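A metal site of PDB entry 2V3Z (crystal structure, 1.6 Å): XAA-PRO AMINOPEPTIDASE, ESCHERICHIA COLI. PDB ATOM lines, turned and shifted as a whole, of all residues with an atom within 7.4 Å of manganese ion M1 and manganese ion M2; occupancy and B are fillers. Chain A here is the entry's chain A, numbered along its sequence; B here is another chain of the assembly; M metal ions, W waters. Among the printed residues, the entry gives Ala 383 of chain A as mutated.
O of Val 1 of chain B is in hydrogen-bond range of NE2 of His 361 (2.6 Å).
OH of Tyr 229 sits close to OD1 of Asp 271 (2.9 Å).
The backbone NH (N) of Glu 406 lies within hydrogen-bond range of the backbone carbonyl oxygen (O) of Thr 273 (2.9 Å).
O of His 354 is in hydrogen-bond range of N of Thr 381 (2.9 Å).
OD2 of Asp 260 sits close to OG1 of Thr 273, at 3.1 Å.
The backbone NH (N) of Asp 260 is in hydrogen-bond range of the backbone carbonyl oxygen (O) of Ile 232 (2.9 Å).
The side-chain hydroxyl (OH) of Tyr 229 sits close to the backbone NH (N) of Ala 261 (3.0 Å).
The backbone carbonyl oxygen (O) of Thr 381 sits at hydrogen-bond distance from the side-chain hydroxyl (OG) of Ser 353 (2.6 Å).
Tyr 229 touches manganese ion M1 (OH to MN, 3.6 Å).
Thr 273 touches manganese ion M1 (OG1 to MN, 3.5 Å).
Of the 27 residues printed, 6 come within 4 Å of manganese ion M1.
CG2 of Thr 381 touches manganese ion M2 (3.99 Å).
Along chain A the residues within 4 Å of manganese ion M2 span positions 271 to 406.
The nearest printed residue that does not touch manganese ion M2 is Pro 2 of chain B (4.1 Å).
Manganese ion M1 is bound by the backbone nitrogen of Val 1 of chain B (1.8 Å), the side-chain carboxylate of Asp 271 (1.9 Å), the side-chain carboxylate of Glu 406 (2.0 Å) and the side-chain carboxylate of Asp 260 (2.1 Å).
Manganese ion M1 has four donor atoms within binding distance.
Slightly farther from manganese ion M1 lies OD2 of Asp 260 (2.7 Å).
N of Val 1 of chain B is bound to manganese ion M2 (1.9 Å).
The side-chain carboxylate (OD2) of Asp 271 is bound to manganese ion M2 (2.1 Å).
A ring nitrogen (NE2) of His 354 is bound to manganese ion M2.
OE2 of Glu 406 binds manganese ion M2 (2.5 Å).
Manganese ion M2 has four donor atoms within binding distance.
Slightly farther from manganese ion M2 lies the backbone carbonyl oxygen (O) of Val 1 of chain B (2.8 Å).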
ATOM      1  N   TYR A 229     -19.137  15.219   8.978  1.00  0.00           N
ATOM      2  CA  TYR A 229     -19.772  16.456   8.547  1.00  0.00           C
ATOM      3  C   TYR A 229     -18.667  17.481   8.410  1.00  0.00           C
ATOM      4  O   TYR A 229     -17.581  17.295   8.919  1.00  0.00           O
ATOM      5  CB  TYR A 229     -20.842  16.942   9.505  1.00  0.00           C
ATOM      6  CG  TYR A 229     -20.383  17.109  10.914  1.00  0.00           C
ATOM      7  CD1 TYR A 229     -20.337  16.021  11.782  1.00  0.00           C
ATOM      8  CD2 TYR A 229     -19.938  18.338  11.420  1.00  0.00           C
ATOM      9  CE1 TYR A 229     -19.880  16.133  13.076  1.00  0.00           C
ATOM     10  CE2 TYR A 229     -19.489  18.454  12.711  1.00  0.00           C
ATOM     11  CZ  TYR A 229     -19.424  17.353  13.534  1.00  0.00           C
ATOM     12  OH  TYR A 229     -18.989  17.466  14.829  1.00  0.00           O
ATOM     13  N   ILE A 232     -16.468  22.671  11.746  1.00  0.00           N
ATOM     14  CA  ILE A 232     -16.736  24.065  12.129  1.00  0.00           C
ATOM     15  C   ILE A 232     -15.635  24.550  13.074  1.00  0.00           C
ATOM     16  O   ILE A 232     -15.400  23.911  14.115  1.00  0.00           O
ATOM     17  CB  ILE A 232     -18.102  24.101  12.857  1.00  0.00           C
ATOM     18  CG1 ILE A 232     -19.228  23.755  11.889  1.00  0.00           C
ATOM     19  CG2 ILE A 232     -18.352  25.425  13.585  1.00  0.00           C
ATOM     20  CD1 ILE A 232     -20.464  23.090  12.529  1.00  0.00           C
ATOM     21  N   ILE A 259     -15.077  24.664  18.239  1.00  0.00           N
ATOM     22  CA  ILE A 259     -14.767  23.634  17.249  1.00  0.00           C
ATOM     23  C   ILE A 259     -15.847  22.576  17.371  1.00  0.00           C
ATOM     24  O   ILE A 259     -16.014  21.966  18.414  1.00  0.00           O
ATOM     25  CB  ILE A 259     -13.407  23.005  17.458  1.00  0.00           C
ATOM     26  CG1 ILE A 259     -12.320  24.093  17.431  1.00  0.00           C
ATOM     27  CG2 ILE A 259     -13.165  21.913  16.423  1.00  0.00           C
ATOM     28  CD1 ILE A 259     -10.920  23.518  17.458  1.00  0.00           C
ATOM     29  N   ASP A 260     -16.593  22.362  16.277  1.00  0.00           N
ATOM     30  CA  ASP A 260     -17.590  21.275  16.182  1.00  0.00           C
ATOM     31  C   ASP A 260     -17.093  20.384  15.050  1.00  0.00           C
ATOM     32  O   ASP A 260     -17.054  20.776  13.911  1.00  0.00           O
ATOM     33  CB  ASP A 260     -18.962  21.904  15.903  1.00  0.00           C
ATOM     34  CG  ASP A 260     -20.131  20.954  16.099  1.00  0.00           C
ATOM     35  OD1 ASP A 260     -19.894  19.735  16.110  1.00  0.00           O
ATOM     36  OD2 ASP A 260     -21.266  21.475  16.277  1.00  0.00           O
ATOM     37  N   ALA A 261     -16.634  19.196  15.425  1.00  0.00           N
ATOM     38  CA  ALA A 261     -16.014  18.300  14.479  1.00  0.00           C
ATOM     39  C   ALA A 261     -16.222  16.862  14.918  1.00  0.00           C
ATOM     40  O   ALA A 261     -16.241  16.551  16.102  1.00  0.00           O
ATOM     41  CB  ALA A 261     -14.513  18.584  14.362  1.00  0.00           C
ATOM     42  N   GLY A 262     -16.370  15.980  13.945  1.00  0.00           N
ATOM     43  CA  GLY A 262     -16.556  14.571  14.227  1.00  0.00           C
ATOM     44  C   GLY A 262     -16.062  13.704  13.100  1.00  0.00           C
ATOM     45  O   GLY A 262     -16.133  14.103  11.925  1.00  0.00           O
ATOM     46  N   GLY A 270     -18.868  10.302  14.943  1.00  0.00           N
ATOM     47  CA  GLY A 270     -18.649  11.053  16.147  1.00  0.00           C
ATOM     48  C   GLY A 270     -19.120  12.503  15.952  1.00  0.00           C
ATOM     49  O   GLY A 270     -19.278  12.978  14.838  1.00  0.00           O
ATOM     50  N   ASP A 271     -19.317  13.248  17.040  1.00  0.00           N
ATOM     51  CA  ASP A 271     -19.838  14.628  16.960  1.00  0.00           C
ATOM     52  C   ASP A 271     -19.545  15.290  18.284  1.00  0.00           C
ATOM     53  O   ASP A 271     -20.292  15.140  19.237  1.00  0.00           O
ATOM     54  CB  ASP A 271     -21.334  14.623  16.639  1.00  0.00           C
ATOM     55  CG  ASP A 271     -21.905  15.973  16.496  1.00  0.00           C
ATOM     56  OD1 ASP A 271     -21.160  16.948  16.685  1.00  0.00           O
ATOM     57  OD2 ASP A 271     -23.125  16.071  16.213  1.00  0.00           O
ATOM     58  N   ILE A 272     -18.431  16.034  18.378  1.00  0.00           N
ATOM     59  CA  ILE A 272     -18.052  16.744  19.589  1.00  0.00           C
ATOM     60  C   ILE A 272     -17.946  18.216  19.283  1.00  0.00           C
ATOM     61  O   ILE A 272     -17.494  18.625  18.208  1.00  0.00           O
ATOM     62  CB  ILE A 272     -16.688  16.266  20.114  1.00  0.00           C
ATOM     63  CG1 ILE A 272     -16.781  14.812  20.555  1.00  0.00           C
ATOM     64  CG2 ILE A 272     -16.157  17.163  21.254  1.00  0.00           C
ATOM     65  CD1 ILE A 272     -15.461  14.236  21.096  1.00  0.00           C
ATOM     66  N   THR A 273     -18.362  19.030  20.257  1.00  0.00           N
ATOM     67  CA  THR A 273     -18.028  20.467  20.239  1.00  0.00           C
ATOM     68  C   THR A 273     -17.265  20.795  21.515  1.00  0.00           C
ATOM     69  O   THR A 273     -17.683  20.402  22.612  1.00  0.00           O
ATOM     70  CB  THR A 273     -19.227  21.406  20.144  1.00  0.00           C
ATOM     71  OG1 THR A 273     -20.058  21.035  19.043  1.00  0.00           O
ATOM     72  CG2 THR A 273     -18.802  22.848  19.930  1.00  0.00           C
ATOM     73  N   LEU A 352     -31.261  20.735  21.937  1.00  0.00           N
ATOM     74  CA  LEU A 352     -30.232  20.180  22.824  1.00  0.00           C
ATOM     75  C   LEU A 352     -29.574  18.915  22.275  1.00  0.00           C
ATOM     76  O   LEU A 352     -28.379  18.685  22.493  1.00  0.00           O
ATOM     77  CB  LEU A 352     -30.836  19.870  24.183  1.00  0.00           C
ATOM     78  CG  LEU A 352     -29.897  19.354  25.279  1.00  0.00           C
ATOM     79  CD1 LEU A 352     -28.895  20.430  25.691  1.00  0.00           C
ATOM     80  CD2 LEU A 352     -30.737  18.917  26.464  1.00  0.00           C
ATOM     81  N   SER A 353     -30.352  18.084  21.586  1.00  0.00           N
ATOM     82  CA  SER A 353     -29.922  16.729  21.274  1.00  0.00           C
ATOM     83  C   SER A 353     -30.475  16.236  19.968  1.00  0.00           C
ATOM     84  O   SER A 353     -31.634  16.517  19.654  1.00  0.00           O
ATOM     85  CB  SER A 353     -30.423  15.761  22.351  1.00  0.00           C
ATOM     86  OG  SER A 353     -29.825  16.025  23.607  1.00  0.00           O
ATOM     87  N   HIS A 354     -29.668  15.492  19.247  1.00  0.00           N
ATOM     88  CA  HIS A 354     -30.130  14.766  18.072  1.00  0.00           C
ATOM     89  C   HIS A 354     -29.607  13.349  18.132  1.00  0.00           C
ATOM     90  O   HIS A 354     -28.556  13.065  18.740  1.00  0.00           O
ATOM     91  CB  HIS A 354     -29.680  15.447  16.763  1.00  0.00           C
ATOM     92  CG  HIS A 354     -28.212  15.653  16.613  1.00  0.00           C
ATOM     93  ND1 HIS A 354     -27.339  14.661  16.208  1.00  0.00           N
ATOM     94  CD2 HIS A 354     -27.453  16.777  16.768  1.00  0.00           C
ATOM     95  CE1 HIS A 354     -26.103  15.153  16.142  1.00  0.00           C
ATOM     96  NE2 HIS A 354     -26.151  16.425  16.479  1.00  0.00           N
ATOM     97  N   TRP A 355     -30.312  12.419  17.476  1.00  0.00           N
ATOM     98  CA  TRP A 355     -29.820  11.069  17.348  1.00  0.00           C
ATOM     99  C   TRP A 355     -28.482  11.030  16.597  1.00  0.00           C
ATOM    100  O   TRP A 355     -28.248  11.879  15.735  1.00  0.00           O
ATOM    101  CB  TRP A 355     -30.800  10.177  16.573  1.00  0.00           C
ATOM    102  CG  TRP A 355     -32.239  10.204  16.997  1.00  0.00           C
ATOM    103  CD1 TRP A 355     -33.295  10.379  16.174  1.00  0.00           C
ATOM    104  CD2 TRP A 355     -32.789   9.966  18.307  1.00  0.00           C
ATOM    105  NE1 TRP A 355     -34.478  10.268  16.871  1.00  0.00           N
ATOM    106  CE2 TRP A 355     -34.199  10.009  18.181  1.00  0.00           C
ATOM    107  CE3 TRP A 355     -32.236   9.678  19.559  1.00  0.00           C
ATOM    108  CZ2 TRP A 355     -35.054   9.849  19.267  1.00  0.00           C
ATOM    109  CZ3 TRP A 355     -33.093   9.511  20.638  1.00  0.00           C
ATOM    110  CH2 TRP A 355     -34.493   9.590  20.491  1.00  0.00           C
ATOM    111  N   LEU A 356     -27.702   9.988  16.837  1.00  0.00           N
ATOM    112  CA  LEU A 356     -26.355   9.839  16.249  1.00  0.00           C
ATOM    113  C   LEU A 356     -26.223   8.406  15.738  1.00  0.00           C
ATOM    114  O   LEU A 356     -26.648   7.458  16.423  1.00  0.00           O
ATOM    115  CB  LEU A 356     -25.300  10.177  17.300  1.00  0.00           C
ATOM    116  CG  LEU A 356     -23.849  10.290  16.879  1.00  0.00           C
ATOM    117  CD1 LEU A 356     -23.672  11.558  15.994  1.00  0.00           C
ATOM    118  CD2 LEU A 356     -22.995  10.354  18.163  1.00  0.00           C
ATOM    119  N   VAL A 360     -24.831  11.799  11.054  1.00  0.00           N
ATOM    120  CA  VAL A 360     -24.649  12.664  12.235  1.00  0.00           C
ATOM    121  C   VAL A 360     -25.968  13.162  12.791  1.00  0.00           C
ATOM    122  O   VAL A 360     -26.167  13.141  14.006  1.00  0.00           O
ATOM    123  CB  VAL A 360     -23.620  13.800  12.014  1.00  0.00           C
ATOM    124  CG1 VAL A 360     -24.044  14.735  10.959  1.00  0.00           C
ATOM    125  CG2 VAL A 360     -23.324  14.506  13.351  1.00  0.00           C
ATOM    126  N   HIS A 361     -26.881  13.565  11.913  1.00  0.00           N
ATOM    127  CA  HIS A 361     -28.272  13.803  12.309  1.00  0.00           C
ATOM    128  C   HIS A 361     -29.028  12.527  11.965  1.00  0.00           C
ATOM    129  O   HIS A 361     -29.545  12.345  10.857  1.00  0.00           O
ATOM    130  CB  HIS A 361     -28.867  15.000  11.605  1.00  0.00           C
ATOM    131  CG  HIS A 361     -28.262  16.292  12.032  1.00  0.00           C
ATOM    132  ND1 HIS A 361     -28.396  17.440  11.284  1.00  0.00           N
ATOM    133  CD2 HIS A 361     -27.522  16.609  13.097  1.00  0.00           C
ATOM    134  CE1 HIS A 361     -27.758  18.428  11.905  1.00  0.00           C
ATOM    135  NE2 HIS A 361     -27.206  17.950  13.006  1.00  0.00           N
ATOM    136  N   THR A 381     -26.605  13.142  20.855  1.00  0.00           N
ATOM    137  CA  THR A 381     -25.719  14.202  21.296  1.00  0.00           C
ATOM    138  C   THR A 381     -26.387  14.993  22.417  1.00  0.00           C
ATOM    139  O   THR A 381     -27.615  14.964  22.607  1.00  0.00           O
ATOM    140  CB  THR A 381     -25.392  15.149  20.175  1.00  0.00           C
ATOM    141  OG1 THR A 381     -26.611  15.774  19.702  1.00  0.00           O
ATOM    142  CG2 THR A 381     -24.682  14.402  19.047  1.00  0.00           C
ATOM    143  N   VAL A 382     -25.565  15.744  23.151  1.00  0.00           N
ATOM    144  CA  VAL A 382     -26.040  16.646  24.186  1.00  0.00           C
ATOM    145  C   VAL A 382     -25.215  17.922  23.977  1.00  0.00           C
ATOM    146  O   VAL A 382     -24.010  17.886  24.202  1.00  0.00           O
ATOM    147  CB  VAL A 382     -25.793  16.091  25.577  1.00  0.00           C
ATOM    148  CG1 VAL A 382     -26.451  16.996  26.629  1.00  0.00           C
ATOM    149  CG2 VAL A 382     -26.307  14.623  25.673  1.00  0.00           C
ATOM    150  N   ALA A 383     -25.853  19.016  23.545  1.00  0.00           N
ATOM    151  CA  ALA A 383     -25.131  20.159  23.001  1.00  0.00           C
ATOM    152  C   ALA A 383     -25.755  21.491  23.329  1.00  0.00           C
ATOM    153  O   ALA A 383     -26.204  22.214  22.454  1.00  0.00           O
ATOM    154  CB  ALA A 383     -25.049  20.006  21.478  1.00  0.00           C
ATOM    155  N   ARG A 404     -20.469  26.520  22.670  1.00  0.00           N
ATOM    156  CA  ARG A 404     -21.221  25.281  22.640  1.00  0.00           C
ATOM    157  C   ARG A 404     -20.289  24.196  23.186  1.00  0.00           C
ATOM    158  O   ARG A 404     -19.080  24.213  22.926  1.00  0.00           O
ATOM    159  CB  ARG A 404     -21.664  24.919  21.210  1.00  0.00           C
ATOM    160  CG  ARG A 404     -22.404  23.573  21.101  1.00  0.00           C
ATOM    161  CD  ARG A 404     -23.173  23.454  19.791  1.00  0.00           C
ATOM    162  NE  ARG A 404     -22.366  23.443  18.554  1.00  0.00           N
ATOM    163  CZ  ARG A 404     -22.287  24.445  17.672  1.00  0.00           C
ATOM    164  NH1 ARG A 404     -22.831  25.621  17.891  1.00  0.00           N
ATOM    165  NH2 ARG A 404     -21.604  24.272  16.522  1.00  0.00           N
ATOM    166  N   GLU A 406     -20.432  19.943  23.565  1.00  0.00           N
ATOM    167  CA  GLU A 406     -21.248  18.812  23.088  1.00  0.00           C
ATOM    168  C   GLU A 406     -20.536  17.495  23.295  1.00  0.00           C
ATOM    169  O   GLU A 406     -19.383  17.331  22.854  1.00  0.00           O
ATOM    170  CB  GLU A 406     -21.539  19.016  21.623  1.00  0.00           C
ATOM    171  CG  GLU A 406     -22.223  17.868  20.896  1.00  0.00           C
ATOM    172  CD  GLU A 406     -22.549  18.259  19.464  1.00  0.00           C
ATOM    173  OE1 GLU A 406     -21.702  18.955  18.823  1.00  0.00           O
ATOM    174  OE2 GLU A 406     -23.621  17.860  18.975  1.00  0.00           O
ATOM    175  N   ASP A 407     -21.278  16.548  23.874  1.00  0.00           N
ATOM    176  CA  ASP A 407     -20.809  15.168  24.057  1.00  0.00           C
ATOM    177  C   ASP A 407     -21.786  14.226  23.359  1.00  0.00           C
ATOM    178  O   ASP A 407     -22.927  14.583  23.053  1.00  0.00           O
ATOM    179  CB  ASP A 407     -20.742  14.816  25.551  1.00  0.00           C
ATOM    180  CG  ASP A 407     -19.431  15.254  26.240  1.00  0.00           C
ATOM    181  OD1 ASP A 407     -18.382  15.418  25.534  1.00  0.00           O
ATOM    182  OD2 ASP A 407     -19.450  15.420  27.478  1.00  0.00           O
ATOM    183  N   ASP A 408     -21.322  13.006  23.121  1.00  0.00           N
ATOM    184  CA  ASP A 408     -22.158  11.926  22.555  1.00  0.00           C
ATOM    185  C   ASP A 408     -22.376  10.877  23.623  1.00  0.00           C
ATOM    186  O   ASP A 408     -21.428  10.440  24.292  1.00  0.00           O
ATOM    187  CB  ASP A 408     -21.423  11.253  21.409  1.00  0.00           C
ATOM    188  CG  ASP A 408     -20.988  12.232  20.343  1.00  0.00           C
ATOM    189  OD1 ASP A 408     -21.671  13.290  20.216  1.00  0.00           O
ATOM    190  OD2 ASP A 408     -19.962  11.969  19.662  1.00  0.00           O
ATOM    191  N   VAL B   1     -23.282  18.986  16.031  1.00  0.00           N
ATOM    192  CA  VAL B   1     -23.639  19.943  14.934  1.00  0.00           C
ATOM    193  C   VAL B   1     -25.119  20.160  15.066  1.00  0.00           C
ATOM    194  O   VAL B   1     -25.887  19.214  14.921  1.00  0.00           O
ATOM    195  CB  VAL B   1     -23.185  19.447  13.535  1.00  0.00           C
ATOM    196  CG1 VAL B   1     -23.678  18.042  13.260  1.00  0.00           C
ATOM    197  CG2 VAL B   1     -23.639  20.390  12.405  1.00  0.00           C
ATOM    198  N   PRO B   2     -25.527  21.382  15.420  1.00  0.00           N
ATOM    199  CA  PRO B   2     -26.894  21.625  15.822  1.00  0.00           C
ATOM    200  C   PRO B   2     -27.937  21.243  14.784  1.00  0.00           C
ATOM    201  O   PRO B   2     -27.753  21.482  13.582  1.00  0.00           O
ATOM    202  CB  PRO B   2     -26.922  23.146  16.056  1.00  0.00           C
ATOM    203  CG  PRO B   2     -25.517  23.482  16.387  1.00  0.00           C
ATOM    204  CD  PRO B   2     -24.693  22.591  15.554  1.00  0.00           C
ATOM    205  N   LEU B   3     -29.020  20.662  15.283  1.00  0.00           N
ATOM    206  CA  LEU B   3     -30.246  20.435  14.561  1.00  0.00           C
ATOM    207  C   LEU B   3     -31.311  21.378  15.174  1.00  0.00           C
ATOM    208  O   LEU B   3     -32.109  21.949  14.442  1.00  0.00           O
ATOM    209  CB  LEU B   3     -30.659  18.970  14.699  1.00  0.00           C
ATOM    210  CG  LEU B   3     -31.865  18.464  13.938  1.00  0.00           C
ATOM    211  CD1 LEU B   3     -31.699  18.634  12.428  1.00  0.00           C
ATOM    212  CD2 LEU B   3     -32.098  17.000  14.306  1.00  0.00           C
ATOM    213  OXT LEU B   3     -31.389  21.635  16.400  1.00  0.00           O
HETATM  214 MN    MN M   1     -21.654  18.825  16.792  1.00  0.00          MN
HETATM  215 MN    MN M   2     -24.432  17.589  16.658  1.00  0.00          MN
HETATM  216  O   HOH W   1     -25.395  19.933  18.249  1.00  0.00           O
